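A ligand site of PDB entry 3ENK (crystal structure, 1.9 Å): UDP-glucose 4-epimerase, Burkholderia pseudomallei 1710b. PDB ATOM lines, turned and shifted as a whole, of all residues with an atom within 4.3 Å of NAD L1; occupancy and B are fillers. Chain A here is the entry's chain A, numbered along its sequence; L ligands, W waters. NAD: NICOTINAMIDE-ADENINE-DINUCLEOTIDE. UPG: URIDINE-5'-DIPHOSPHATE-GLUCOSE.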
ATOM      1  N   GLY A  12      31.677 -32.732  13.192  1.00  0.00           N
ATOM      2  CA  GLY A  12      30.296 -32.638  13.637  1.00  0.00           C
ATOM      3  C   GLY A  12      29.368 -33.399  12.705  1.00  0.00           C
ATOM      4  O   GLY A  12      28.202 -33.127  12.655  1.00  0.00           O
ATOM      5  N   ALA A  14      28.026 -36.399  12.788  1.00  0.00           N
ATOM      6  CA  ALA A  14      26.918 -37.174  13.391  1.00  0.00           C
ATOM      7  C   ALA A  14      25.695 -36.327  13.724  1.00  0.00           C
ATOM      8  O   ALA A  14      24.612 -36.865  14.009  1.00  0.00           O
ATOM      9  CB  ALA A  14      27.386 -37.912  14.650  1.00  0.00           C
ATOM     10  N   GLY A  15      25.862 -34.999  13.660  1.00  0.00           N
ATOM     11  CA  GLY A  15      24.754 -34.096  13.982  1.00  0.00           C
ATOM     12  C   GLY A  15      23.775 -33.949  12.852  1.00  0.00           C
ATOM     13  O   GLY A  15      23.853 -34.661  11.847  1.00  0.00           O
ATOM     14  N   TYR A  16      22.850 -33.004  13.009  1.00  0.00           N
ATOM     15  CA  TYR A  16      21.705 -32.841  12.093  1.00  0.00           C
ATOM     16  C   TYR A  16      22.125 -32.467  10.657  1.00  0.00           C
ATOM     17  O   TYR A  16      21.903 -33.240   9.693  1.00  0.00           O
ATOM     18  CB  TYR A  16      20.770 -31.785  12.694  1.00  0.00           C
ATOM     19  CG  TYR A  16      19.570 -31.388  11.864  1.00  0.00           C
ATOM     20  CD1 TYR A  16      18.836 -32.346  11.130  1.00  0.00           C
ATOM     21  CD2 TYR A  16      19.166 -30.062  11.807  1.00  0.00           C
ATOM     22  CE1 TYR A  16      17.713 -31.980  10.392  1.00  0.00           C
ATOM     23  CE2 TYR A  16      18.053 -29.677  11.048  1.00  0.00           C
ATOM     24  CZ  TYR A  16      17.335 -30.629  10.346  1.00  0.00           C
ATOM     25  OH  TYR A  16      16.220 -30.251   9.618  1.00  0.00           O
ATOM     26  N   ILE A  17      22.786 -31.320  10.501  1.00  0.00           N
ATOM     27  CA  ILE A  17      23.123 -30.868   9.161  1.00  0.00           C
ATOM     28  C   ILE A  17      24.289 -31.673   8.606  1.00  0.00           C
ATOM     29  O   ILE A  17      24.347 -31.939   7.412  1.00  0.00           O
ATOM     30  CB  ILE A  17      23.409 -29.339   9.105  1.00  0.00           C
ATOM     31  CG1 ILE A  17      22.301 -28.552   9.819  1.00  0.00           C
ATOM     32  CG2 ILE A  17      23.631 -28.890   7.601  1.00  0.00           C
ATOM     33  CD1 ILE A  17      22.583 -27.039  10.036  1.00  0.00           C
ATOM     34  N   GLY A  18      25.228 -32.044   9.466  1.00  0.00           N
ATOM     35  CA  GLY A  18      26.392 -32.769   9.015  1.00  0.00           C
ATOM     36  C   GLY A  18      26.039 -34.158   8.498  1.00  0.00           C
ATOM     37  O   GLY A  18      26.606 -34.615   7.497  1.00  0.00           O
ATOM     38  N   ALA A  35      34.244 -36.808  12.047  1.00  0.00           N
ATOM     39  CA  ALA A  35      34.839 -36.637  13.371  1.00  0.00           C
ATOM     40  C   ALA A  35      33.786 -35.988  14.254  1.00  0.00           C
ATOM     41  O   ALA A  35      33.327 -34.875  13.955  1.00  0.00           O
ATOM     42  CB  ALA A  35      36.067 -35.768  13.259  1.00  0.00           C
ATOM     43  N   ASP A  36      33.343 -36.685  15.308  1.00  0.00           N
ATOM     44  CA  ASP A  36      32.258 -36.126  16.143  1.00  0.00           C
ATOM     45  C   ASP A  36      32.424 -36.712  17.539  1.00  0.00           C
ATOM     46  O   ASP A  36      32.559 -37.927  17.678  1.00  0.00           O
ATOM     47  CB  ASP A  36      30.877 -36.493  15.564  1.00  0.00           C
ATOM     48  CG  ASP A  36      29.753 -35.605  16.077  1.00  0.00           C
ATOM     49  OD1 ASP A  36      29.079 -34.981  15.227  1.00  0.00           O
ATOM     50  OD2 ASP A  36      29.541 -35.489  17.316  1.00  0.00           O
ATOM     51  N   ASN A  37      32.435 -35.863  18.564  1.00  0.00           N
ATOM     52  CA  ASN A  37      32.535 -36.348  19.955  1.00  0.00           C
ATOM     53  C   ASN A  37      31.203 -36.695  20.601  1.00  0.00           C
ATOM     54  O   ASN A  37      31.152 -37.005  21.810  1.00  0.00           O
ATOM     55  CB  ASN A  37      33.346 -35.386  20.829  1.00  0.00           C
ATOM     56  CG  ASN A  37      32.618 -34.068  21.080  1.00  0.00           C
ATOM     57  OD1 ASN A  37      31.560 -33.839  20.520  1.00  0.00           O
ATOM     58  ND2 ASN A  37      33.175 -33.227  21.934  1.00  0.00           N
ATOM     59  N   LEU A  38      30.118 -36.664  19.802  1.00  0.00           N
ATOM     60  CA  LEU A  38      28.768 -37.076  20.219  1.00  0.00           C
ATOM     61  C   LEU A  38      28.243 -36.300  21.422  1.00  0.00           C
ATOM     62  O   LEU A  38      27.389 -36.789  22.193  1.00  0.00           O
ATOM     63  CB  LEU A  38      28.714 -38.602  20.492  1.00  0.00           C
ATOM     64  CG  LEU A  38      29.264 -39.424  19.305  1.00  0.00           C
ATOM     65  CD1 LEU A  38      29.289 -40.902  19.634  1.00  0.00           C
ATOM     66  CD2 LEU A  38      28.472 -39.176  17.987  1.00  0.00           C
ATOM     67  N   VAL A  39      28.729 -35.077  21.583  1.00  0.00           N
ATOM     68  CA  VAL A  39      28.251 -34.185  22.642  1.00  0.00           C
ATOM     69  C   VAL A  39      26.747 -33.795  22.434  1.00  0.00           C
ATOM     70  O   VAL A  39      26.025 -33.566  23.406  1.00  0.00           O
ATOM     71  CB  VAL A  39      29.243 -32.975  22.850  1.00  0.00           C
ATOM     72  CG1 VAL A  39      29.194 -31.976  21.668  1.00  0.00           C
ATOM     73  CG2 VAL A  39      29.021 -32.255  24.162  1.00  0.00           C
ATOM     74  N   ASN A  40      26.264 -33.758  21.197  1.00  0.00           N
ATOM     75  CA  ASN A  40      24.868 -33.439  20.927  1.00  0.00           C
ATOM     76  C   ASN A  40      24.265 -34.386  19.883  1.00  0.00           C
ATOM     77  O   ASN A  40      23.311 -34.057  19.146  1.00  0.00           O
ATOM     78  CB  ASN A  40      24.729 -31.946  20.503  1.00  0.00           C
ATOM     79  CG  ASN A  40      23.299 -31.445  20.608  1.00  0.00           C
ATOM     80  OD1 ASN A  40      22.578 -31.797  21.554  1.00  0.00           O
ATOM     81  ND2 ASN A  40      22.867 -30.657  19.621  1.00  0.00           N
ATOM     82  N   SER A  41      24.807 -35.594  19.795  1.00  0.00           N
ATOM     83  CA  SER A  41      24.340 -36.519  18.775  1.00  0.00           C
ATOM     84  C   SER A  41      24.609 -37.941  19.218  1.00  0.00           C
ATOM     85  O   SER A  41      25.245 -38.159  20.224  1.00  0.00           O
ATOM     86  CB  SER A  41      25.014 -36.272  17.438  1.00  0.00           C
ATOM     87  OG  SER A  41      26.428 -36.243  17.593  1.00  0.00           O
ATOM     88  N   THR A  62      35.819 -38.200  18.243  1.00  0.00           N
ATOM     89  CA  THR A  62      36.985 -37.374  18.521  1.00  0.00           C
ATOM     90  C   THR A  62      36.539 -35.948  18.835  1.00  0.00           C
ATOM     91  O   THR A  62      35.771 -35.361  18.069  1.00  0.00           O
ATOM     92  CB  THR A  62      37.900 -37.357  17.269  1.00  0.00           C
ATOM     93  OG1 THR A  62      38.386 -38.682  17.002  1.00  0.00           O
ATOM     94  CG2 THR A  62      39.093 -36.446  17.442  1.00  0.00           C
ATOM     95  N   ASP A  63      37.023 -35.388  19.946  1.00  0.00           N
ATOM     96  CA  ASP A  63      36.899 -33.962  20.195  1.00  0.00           C
ATOM     97  C   ASP A  63      37.888 -33.255  19.261  1.00  0.00           C
ATOM     98  O   ASP A  63      39.124 -33.332  19.435  1.00  0.00           O
ATOM     99  CB  ASP A  63      37.180 -33.640  21.675  1.00  0.00           C
ATOM    100  CG  ASP A  63      37.090 -32.152  21.993  1.00  0.00           C
ATOM    101  OD1 ASP A  63      37.001 -31.317  21.071  1.00  0.00           O
ATOM    102  OD2 ASP A  63      37.164 -31.816  23.187  1.00  0.00           O
ATOM    103  N   VAL A  64      37.350 -32.555  18.259  1.00  0.00           N
ATOM    104  CA  VAL A  64      38.224 -31.965  17.231  1.00  0.00           C
ATOM    105  C   VAL A  64      39.089 -30.786  17.740  1.00  0.00           C
ATOM    106  O   VAL A  64      40.032 -30.389  17.037  1.00  0.00           O
ATOM    107  CB  VAL A  64      37.485 -31.642  15.872  1.00  0.00           C
ATOM    108  CG1 VAL A  64      36.602 -32.816  15.441  1.00  0.00           C
ATOM    109  CG2 VAL A  64      36.695 -30.409  15.962  1.00  0.00           C
ATOM    110  N   PHE A  85      31.224 -28.520  10.747  1.00  0.00           N
ATOM    111  CA  PHE A  85      29.959 -28.373  11.473  1.00  0.00           C
ATOM    112  C   PHE A  85      30.065 -28.388  13.000  1.00  0.00           C
ATOM    113  O   PHE A  85      29.111 -28.004  13.712  1.00  0.00           O
ATOM    114  CB  PHE A  85      28.976 -29.517  11.089  1.00  0.00           C
ATOM    115  CG  PHE A  85      28.587 -29.549   9.626  1.00  0.00           C
ATOM    116  CD1 PHE A  85      27.552 -28.748   9.166  1.00  0.00           C
ATOM    117  CD2 PHE A  85      29.190 -30.456   8.754  1.00  0.00           C
ATOM    118  CE1 PHE A  85      27.139 -28.806   7.783  1.00  0.00           C
ATOM    119  CE2 PHE A  85      28.806 -30.527   7.405  1.00  0.00           C
ATOM    120  CZ  PHE A  85      27.779 -29.688   6.913  1.00  0.00           C
ATOM    121  N   ALA A  86      31.199 -28.831  13.534  1.00  0.00           N
ATOM    122  CA  ALA A  86      31.306 -29.066  14.976  1.00  0.00           C
ATOM    123  C   ALA A  86      31.165 -27.735  15.756  1.00  0.00           C
ATOM    124  O   ALA A  86      31.926 -26.802  15.536  1.00  0.00           O
ATOM    125  CB  ALA A  86      32.658 -29.695  15.256  1.00  0.00           C
ATOM    126  N   ALA A  87      30.190 -27.662  16.651  1.00  0.00           N
ATOM    127  CA  ALA A  87      29.968 -26.527  17.517  1.00  0.00           C
ATOM    128  C   ALA A  87      28.848 -26.856  18.468  1.00  0.00           C
ATOM    129  O   ALA A  87      28.019 -27.764  18.194  1.00  0.00           O
ATOM    130  CB  ALA A  87      29.569 -25.263  16.689  1.00  0.00           C
ATOM    131  N   LYS A  89      25.501 -25.097  19.928  1.00  0.00           N
ATOM    132  CA  LYS A  89      24.620 -24.224  19.137  1.00  0.00           C
ATOM    133  C   LYS A  89      23.372 -23.799  19.883  1.00  0.00           C
ATOM    134  O   LYS A  89      22.494 -23.202  19.285  1.00  0.00           O
ATOM    135  CB  LYS A  89      24.203 -24.877  17.799  1.00  0.00           C
ATOM    136  CG  LYS A  89      23.272 -26.133  17.984  1.00  0.00           C
ATOM    137  CD  LYS A  89      22.301 -26.352  16.834  1.00  0.00           C
ATOM    138  CE  LYS A  89      21.390 -27.570  17.059  1.00  0.00           C
ATOM    139  NZ  LYS A  89      20.512 -27.874  15.834  1.00  0.00           N
ATOM    140  N   ASN A 104      34.717 -24.239  23.267  1.00  0.00           N
ATOM    141  CA  ASN A 104      34.452 -25.331  22.323  1.00  0.00           C
ATOM    142  C   ASN A 104      34.444 -24.817  20.879  1.00  0.00           C
ATOM    143  O   ASN A 104      35.043 -25.423  19.984  1.00  0.00           O
ATOM    144  CB  ASN A 104      33.137 -26.023  22.614  1.00  0.00           C
ATOM    145  CG  ASN A 104      32.879 -27.225  21.669  1.00  0.00           C
ATOM    146  OD1 ASN A 104      32.066 -27.158  20.736  1.00  0.00           O
ATOM    147  ND2 ASN A 104      33.581 -28.307  21.922  1.00  0.00           N
ATOM    148  N   SER A 108      37.832 -25.690  18.629  1.00  0.00           N
ATOM    149  CA  SER A 108      37.606 -26.713  17.593  1.00  0.00           C
ATOM    150  C   SER A 108      37.978 -26.190  16.202  1.00  0.00           C
ATOM    151  O   SER A 108      38.603 -26.894  15.407  1.00  0.00           O
ATOM    152  CB  SER A 108      36.138 -27.212  17.590  1.00  0.00           C
ATOM    153  OG  SER A 108      35.218 -26.180  17.256  1.00  0.00           O
ATOM    154  N   SER A 127      30.397 -23.666   8.705  1.00  0.00           N
ATOM    155  CA  SER A 127      29.022 -23.445   9.101  1.00  0.00           C
ATOM    156  C   SER A 127      28.843 -22.130   9.867  1.00  0.00           C
ATOM    157  O   SER A 127      29.090 -22.072  11.081  1.00  0.00           O
ATOM    158  CB  SER A 127      28.531 -24.598  10.013  1.00  0.00           C
ATOM    159  OG  SER A 127      28.737 -25.846   9.376  1.00  0.00           O
ATOM    160  N   SER A 128      28.411 -21.070   9.182  1.00  0.00           N
ATOM    161  CA  SER A 128      28.077 -19.843   9.908  1.00  0.00           C
ATOM    162  C   SER A 128      26.565 -19.740  10.014  1.00  0.00           C
ATOM    163  O   SER A 128      25.851 -20.722   9.739  1.00  0.00           O
ATOM    164  CB  SER A 128      28.724 -18.613   9.249  1.00  0.00           C
ATOM    165  OG  SER A 128      28.596 -17.485  10.106  1.00  0.00           O
ATOM    166  N   SER A 129      26.058 -18.568  10.422  1.00  0.00           N
ATOM    167  CA  SER A 129      24.678 -18.448  10.825  1.00  0.00           C
ATOM    168  C   SER A 129      24.150 -17.038  10.556  1.00  0.00           C
ATOM    169  O   SER A 129      24.921 -16.078  10.608  1.00  0.00           O
ATOM    170  CB  SER A 129      24.555 -18.742  12.317  1.00  0.00           C
ATOM    171  OG  SER A 129      23.274 -18.415  12.826  1.00  0.00           O
ATOM    172  N   TYR A 153      26.734 -17.491  21.514  1.00  0.00           N
ATOM    173  CA  TYR A 153      26.732 -18.381  20.362  1.00  0.00           C
ATOM    174  C   TYR A 153      26.939 -17.570  19.051  1.00  0.00           C
ATOM    175  O   TYR A 153      27.813 -17.903  18.245  1.00  0.00           O
ATOM    176  CB  TYR A 153      25.448 -19.235  20.296  1.00  0.00           C
ATOM    177  CG  TYR A 153      25.291 -19.851  18.943  1.00  0.00           C
ATOM    178  CD1 TYR A 153      24.368 -19.341  18.024  1.00  0.00           C
ATOM    179  CD2 TYR A 153      26.131 -20.891  18.562  1.00  0.00           C
ATOM    180  CE1 TYR A 153      24.253 -19.883  16.752  1.00  0.00           C
ATOM    181  CE2 TYR A 153      26.021 -21.454  17.272  1.00  0.00           C
ATOM    182  CZ  TYR A 153      25.083 -20.942  16.391  1.00  0.00           C
ATOM    183  OH  TYR A 153      24.977 -21.491  15.140  1.00  0.00           O
ATOM    184  N   LYS A 157      30.301 -17.339  16.167  1.00  0.00           N
ATOM    185  CA  LYS A 157      30.241 -17.384  14.691  1.00  0.00           C
ATOM    186  C   LYS A 157      30.906 -16.150  14.043  1.00  0.00           C
ATOM    187  O   LYS A 157      31.672 -16.289  13.100  1.00  0.00           O
ATOM    188  CB  LYS A 157      28.807 -17.581  14.173  1.00  0.00           C
ATOM    189  CG  LYS A 157      28.187 -18.953  14.584  1.00  0.00           C
ATOM    190  CD  LYS A 157      28.994 -20.125  14.028  1.00  0.00           C
ATOM    191  CE  LYS A 157      28.303 -21.480  14.298  1.00  0.00           C
ATOM    192  NZ  LYS A 157      29.181 -22.582  13.734  1.00  0.00           N
ATOM    193  N   TYR A 181      23.776 -20.226   7.219  1.00  0.00           N
ATOM    194  CA  TYR A 181      22.480 -20.887   7.177  1.00  0.00           C
ATOM    195  C   TYR A 181      21.443 -20.029   7.873  1.00  0.00           C
ATOM    196  O   TYR A 181      21.726 -19.337   8.860  1.00  0.00           O
ATOM    197  CB  TYR A 181      22.517 -22.244   7.902  1.00  0.00           C
ATOM    198  CG  TYR A 181      23.734 -23.114   7.660  1.00  0.00           C
ATOM    199  CD1 TYR A 181      24.373 -23.167   6.423  1.00  0.00           C
ATOM    200  CD2 TYR A 181      24.206 -23.924   8.683  1.00  0.00           C
ATOM    201  CE1 TYR A 181      25.509 -24.013   6.242  1.00  0.00           C
ATOM    202  CE2 TYR A 181      25.277 -24.757   8.514  1.00  0.00           C
ATOM    203  CZ  TYR A 181      25.940 -24.793   7.319  1.00  0.00           C
ATOM    204  OH  TYR A 181      27.021 -25.642   7.182  1.00  0.00           O
ATOM    205  N   PHE A 182      20.209 -20.074   7.366  1.00  0.00           N
ATOM    206  CA  PHE A 182      19.105 -19.448   8.083  1.00  0.00           C
ATOM    207  C   PHE A 182      18.477 -20.421   9.077  1.00  0.00           C
ATOM    208  O   PHE A 182      19.108 -20.698  10.118  1.00  0.00           O
ATOM    209  CB  PHE A 182      18.165 -18.680   7.132  1.00  0.00           C
ATOM    210  CG  PHE A 182      18.720 -17.322   6.786  1.00  0.00           C
ATOM    211  CD1 PHE A 182      19.949 -17.223   6.138  1.00  0.00           C
ATOM    212  CD2 PHE A 182      18.081 -16.167   7.221  1.00  0.00           C
ATOM    213  CE1 PHE A 182      20.543 -15.964   5.864  1.00  0.00           C
ATOM    214  CE2 PHE A 182      18.653 -14.883   6.923  1.00  0.00           C
ATOM    215  CZ  PHE A 182      19.877 -14.807   6.256  1.00  0.00           C
ATOM    216  N   PRO A 184      17.387 -24.160   9.215  1.00  0.00           N
ATOM    217  CA  PRO A 184      17.203 -25.489   8.642  1.00  0.00           C
ATOM    218  C   PRO A 184      16.138 -26.297   9.373  1.00  0.00           C
ATOM    219  O   PRO A 184      16.131 -26.333  10.627  1.00  0.00           O
ATOM    220  CB  PRO A 184      18.581 -26.164   8.827  1.00  0.00           C
ATOM    221  CG  PRO A 184      19.521 -25.074   9.130  1.00  0.00           C
ATOM    222  CD  PRO A 184      18.728 -24.001   9.796  1.00  0.00           C
HETATM  223  PA  NAD L   1      24.183 -30.389  15.771  1.00  0.00           P
HETATM  224  O1A NAD L   1      24.402 -30.179  17.232  1.00  0.00           O
HETATM  225  O2A NAD L   1      23.224 -31.481  15.466  1.00  0.00           O
HETATM  226  O5B NAD L   1      25.554 -30.755  15.033  1.00  0.00           O
HETATM  227  C5B NAD L   1      26.777 -30.368  15.623  1.00  0.00           C
HETATM  228  C4B NAD L   1      27.644 -31.597  15.886  1.00  0.00           C
HETATM  229  O4B NAD L   1      28.911 -31.154  16.365  1.00  0.00           O
HETATM  230  C3B NAD L   1      27.086 -32.500  16.983  1.00  0.00           C
HETATM  231  O3B NAD L   1      27.006 -33.809  16.460  1.00  0.00           O
HETATM  232  C2B NAD L   1      28.129 -32.413  18.122  1.00  0.00           C
HETATM  233  O2B NAD L   1      28.331 -33.602  18.872  1.00  0.00           O
HETATM  234  C1B NAD L   1      29.374 -32.027  17.372  1.00  0.00           C
HETATM  235  N9A NAD L   1      30.442 -31.334  18.124  1.00  0.00           N
HETATM  236  C8A NAD L   1      30.295 -30.227  18.900  1.00  0.00           C
HETATM  237  N7A NAD L   1      31.507 -29.893  19.382  1.00  0.00           N
HETATM  238  C5A NAD L   1      32.427 -30.807  18.919  1.00  0.00           C
HETATM  239  C6A NAD L   1      33.802 -30.943  19.113  1.00  0.00           C
HETATM  240  N6A NAD L   1      34.541 -30.130  19.919  1.00  0.00           N
HETATM  241  N1A NAD L   1      34.425 -31.988  18.465  1.00  0.00           N
HETATM  242  C2A NAD L   1      33.747 -32.873  17.661  1.00  0.00           C
HETATM  243  N3A NAD L   1      32.383 -32.763  17.501  1.00  0.00           N
HETATM  244  C4A NAD L   1      31.742 -31.713  18.116  1.00  0.00           C
HETATM  245  O3  NAD L   1      23.728 -29.013  15.129  1.00  0.00           O
HETATM  246  PN  NAD L   1      23.342 -28.766  13.604  1.00  0.00           P
HETATM  247  O1N NAD L   1      21.970 -28.263  13.635  1.00  0.00           O
HETATM  248  O2N NAD L   1      23.749 -29.870  12.665  1.00  0.00           O
HETATM  249  O5D NAD L   1      24.346 -27.545  13.258  1.00  0.00           O
HETATM  250  C5D NAD L   1      25.551 -27.798  12.574  1.00  0.00           C
HETATM  251  C4D NAD L   1      26.341 -26.500  12.420  1.00  0.00           C
HETATM  252  O4D NAD L   1      25.510 -25.532  11.798  1.00  0.00           O
HETATM  253  C3D NAD L   1      26.808 -25.893  13.727  1.00  0.00           C
HETATM  254  O3D NAD L   1      28.071 -25.285  13.477  1.00  0.00           O
HETATM  255  C2D NAD L   1      25.761 -24.823  14.002  1.00  0.00           C
HETATM  256  O2D NAD L   1      26.250 -23.773  14.802  1.00  0.00           O
HETATM  257  C1D NAD L   1      25.442 -24.353  12.578  1.00  0.00           C
HETATM  258  N1N NAD L   1      24.120 -23.754  12.364  1.00  0.00           N
HETATM  259  C2N NAD L   1      22.986 -24.457  12.696  1.00  0.00           C
HETATM  260  C3N NAD L   1      21.747 -23.920  12.456  1.00  0.00           C
HETATM  261  C7N NAD L   1      20.513 -24.637  12.900  1.00  0.00           C
HETATM  262  O7N NAD L   1      19.397 -23.859  13.089  1.00  0.00           O
HETATM  263  N7N NAD L   1      20.517 -25.959  13.083  1.00  0.00           N
HETATM  264  C4N NAD L   1      21.629 -22.653  11.861  1.00  0.00           C
HETATM  265  C5N NAD L   1      22.794 -21.955  11.533  1.00  0.00           C
HETATM  266  C6N NAD L   1      24.042 -22.534  11.746  1.00  0.00           C
HETATM  267  N1  UPG L   2       9.392 -20.362  18.579  1.00  0.00           N
HETATM  268  C2  UPG L   2       8.204 -20.571  19.290  1.00  0.00           C
HETATM  269  N3  UPG L   2       8.116 -21.581  20.126  1.00  0.00           N
HETATM  270  C4  UPG L   2       9.150 -22.441  20.277  1.00  0.00           C
HETATM  271  C5  UPG L   2      10.339 -22.252  19.577  1.00  0.00           C
HETATM  272  C6  UPG L   2      10.433 -21.192  18.708  1.00  0.00           C
HETATM  273  O2  UPG L   2       7.255 -19.790  19.134  1.00  0.00           O
HETATM  274  O4  UPG L   2       9.055 -23.385  21.076  1.00  0.00           O
HETATM  275  C1C UPG L   2       9.465 -19.252  17.633  1.00  0.00           C
HETATM  276  C2C UPG L   2      10.572 -18.243  17.910  1.00  0.00           C
HETATM  277  O2C UPG L   2      10.109 -17.176  18.755  1.00  0.00           O
HETATM  278  C3C UPG L   2      10.969 -17.808  16.508  1.00  0.00           C
HETATM  279  C4C UPG L   2      10.653 -18.985  15.595  1.00  0.00           C
HETATM  280  O4C UPG L   2       9.740 -19.792  16.323  1.00  0.00           O
HETATM  281  O3C UPG L   2      10.189 -16.686  16.052  1.00  0.00           O
HETATM  282  C5C UPG L   2      11.874 -19.841  15.282  1.00  0.00           C
HETATM  283  O5C UPG L   2      12.689 -19.937  16.450  1.00  0.00           O
HETATM  284  PA  UPG L   2      13.813 -21.092  16.563  1.00  0.00           P
HETATM  285  O1A UPG L   2      14.191 -21.184  18.025  1.00  0.00           O
HETATM  286  O2A UPG L   2      13.455 -22.362  15.804  1.00  0.00           O
HETATM  287  O3A UPG L   2      14.963 -20.451  15.652  1.00  0.00           O
HETATM  288  PB  UPG L   2      15.443 -18.908  15.768  1.00  0.00           P
HETATM  289  O1B UPG L   2      15.056 -18.072  14.570  1.00  0.00           O
HETATM  290  O2B UPG L   2      15.302 -18.371  17.174  1.00  0.00           O
HETATM  291  O3B UPG L   2      16.952 -19.132  15.469  1.00  0.00           O
HETATM  292  C1' UPG L   2      17.613 -19.967  16.363  1.00  0.00           C
HETATM  293  C2' UPG L   2      18.145 -20.987  15.371  1.00  0.00           C
HETATM  294  C3' UPG L   2      19.453 -20.534  14.694  1.00  0.00           C
HETATM  295  C4' UPG L   2      20.310 -19.588  15.544  1.00  0.00           C
HETATM  296  C5' UPG L   2      19.493 -18.479  16.195  1.00  0.00           C
HETATM  297  C6' UPG L   2      20.361 -17.506  16.993  1.00  0.00           C
HETATM  298  O2' UPG L   2      18.232 -22.206  16.091  1.00  0.00           O
HETATM  299  O3' UPG L   2      20.231 -21.686  14.396  1.00  0.00           O
HETATM  300  O4' UPG L   2      21.361 -19.042  14.751  1.00  0.00           O
HETATM  301  O5' UPG L   2      18.580 -19.163  17.044  1.00  0.00           O
HETATM  302  O6' UPG L   2      19.588 -16.420  17.550  1.00  0.00           O
HETATM  303  O   HOH W   1      30.980 -25.294  13.175  1.00  0.00           O
HETATM  304  O   HOH W   2      21.795 -33.141  16.990  1.00  0.00           O
HETATM  305  O   HOH W   3      20.647 -19.231  11.679  1.00  0.00           O
HETATM  306  O   HOH W   4      26.011 -31.342  12.061  1.00  0.00           O
HETATM  307  O   HOH W   5      26.000 -29.231  19.223  1.00  0.00           O
HETATM  308  O   HOH W   6      16.760 -24.275  12.444  1.00  0.00           O
HETATM  309  O   HOH W   7      17.814 -27.247  13.851  1.00  0.00           O
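Merely in contact with NAD L1: Gly 12 (3.4 Å), Ala 14 (3.9 Å), Leu 38 (3.7 Å), Thr 62 (3.2 Å), Ala 86 (3.5 Å), Ala 87 (3.4 Å), Ser 127 (3.6 Å), Ser 128 (3.3 Å), Ser 129 (3.7 Å), Tyr 181 (3.4 Å), Phe 182 (3.6 Å) and Pro 184 (3.4 Å). Hydrophobic or aromatic side chains that line NAD L1: Tyr 16, Ile 17, Val 39, Val 64, Ala 86, Ala 87, Tyr 153, Tyr 181 and Pro 184. Of the 30 residues printed, 27 come within 4 Å of NAD L1. The nearest printed residue that does not touch NAD L1 is Ser 108 (4.1 Å).
O3' of UPG L2 is in hydrogen-bond range of O7N of NAD L1, at 2.7 Å.
OH of Tyr 153 sits at hydrogen-bond distance from O2D of NAD L1. The side-chain amino group (NZ) of Lys 89 lies within salt-bridge range of an oxygen (O1N) of NAD L1. OD1 of Asp 36 is in hydrogen-bond range of O3B of NAD L1, 2.7 Å away. O3B of NAD L1 lies within hydrogen-bond range of OG of Ser 41, 2.7 Å away. The backbone NH (N) of Ile 17 lies within hydrogen-bond range of an oxygen (O2N) of NAD L1 (2.8 Å). The side-chain amide nitrogen (ND2) of Asn 104 lies close to a nitrogen (N6A) of NAD L1. The backbone NH (N) of Asn 40 sits at hydrogen-bond distance from an oxygen (O2B) of NAD L1. The side-chain amide nitrogen (ND2) of Asn 40 lies within hydrogen-bond range of an oxygen (O1A) of NAD L1 (2.9 Å). The backbone NH (N) of Tyr 16 is in hydrogen-bond range of an oxygen (O2A) of NAD L1, at 2.9 Å. O3D of NAD L1 is in hydrogen-bond range of O of Phe 85 (2.9 Å). The side-chain amino group (NZ) of Lys 157 sits at hydrogen-bond distance from an oxygen (O3D) of NAD L1 (2.9 Å). The side-chain carboxylate of Asp 63 sits at hydrogen-bond distance from a nitrogen (N6A) of NAD L1 (3.0 Å). N of Val 64 sits at hydrogen-bond distance from N1A of NAD L1 (3.0 Å). An oxygen (O2B) of NAD L1 lies within hydrogen-bond range of the backbone NH (N) of Val 39 (3.1 Å). A nitrogen (N3A) of NAD L1 is in hydrogen-bond range of the backbone NH (N) of Asn 37. The side-chain amide oxygen of Asn 37 sits close to a nitrogen (N3A) of NAD L1 (3.3 Å). The backbone NH (N) of Gly 15 is in hydrogen-bond range of an oxygen (O3B) of NAD L1 (3.3 Å). OG of Ser 129 lies within hydrogen-bond range of O4' of UPG L2, 2.8 Å away.
The side-chain carboxylate (OD2) of Asp 36 sits at hydrogen-bond distance from the side-chain hydroxyl (OG) of Ser 41 (3.2 Å). OD1 of Asp 36 is in hydrogen-bond range of N of Ala 14, 3.0 Å away. The side-chain hydroxyl of Ser 108 lies within hydrogen-bond range of the backbone carbonyl oxygen of Asn 104. The side-chain amino group of Lys 157 sits at hydrogen-bond distance from the backbone carbonyl oxygen of Ser 127 (2.7 Å). The backbone NH (N) of Val 39 lies close to the side-chain amide oxygen (OD1) of Asn 37 (3.3 Å). N of Asn 37 is in hydrogen-bond range of O of Thr 62. N of Tyr 181 lies within hydrogen-bond range of O of Ser 128 (3.3 Å). OH of Tyr 181 sits at hydrogen-bond distance from OG of Ser 127.
Water W5 lies within hydrogen-bond range of O of Ala 87 (2.7 Å), O1A of NAD L1 (2.7 Å) and ND2 of Asn 40 (3.5 Å). Water W6 bridges an oxygen (O7N) of NAD L1 and the backbone carbonyl oxygen of Pro 184. Water W4 lies within hydrogen-bond range of an oxygen (O2N) of NAD L1 (2.8 Å), the backbone NH of Gly 18 (2.8 Å) and the backbone carbonyl oxygen of Gly 12 (2.9 Å). Water W1 lies within hydrogen-bond range of an oxygen (O3D) of NAD L1 (2.9 Å), the backbone carbonyl oxygen (O) of Ala 86 (3.0 Å), the side-chain amino group (NZ) of Lys 157 (3.3 Å) and the backbone carbonyl oxygen (O) of Phe 85 (3.3 Å). Water W7 bridges a nitrogen (N7N) of NAD L1 (3.1 Å) and the side-chain amino group of Lys 89 (3.4 Å). Water W3 lies within hydrogen-bond range of O of Phe 182 (2.6 Å), OG of Ser 129 (3.0 Å), O of Tyr 181 (3.0 Å) and O4' of UPG L2 (3.2 Å).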
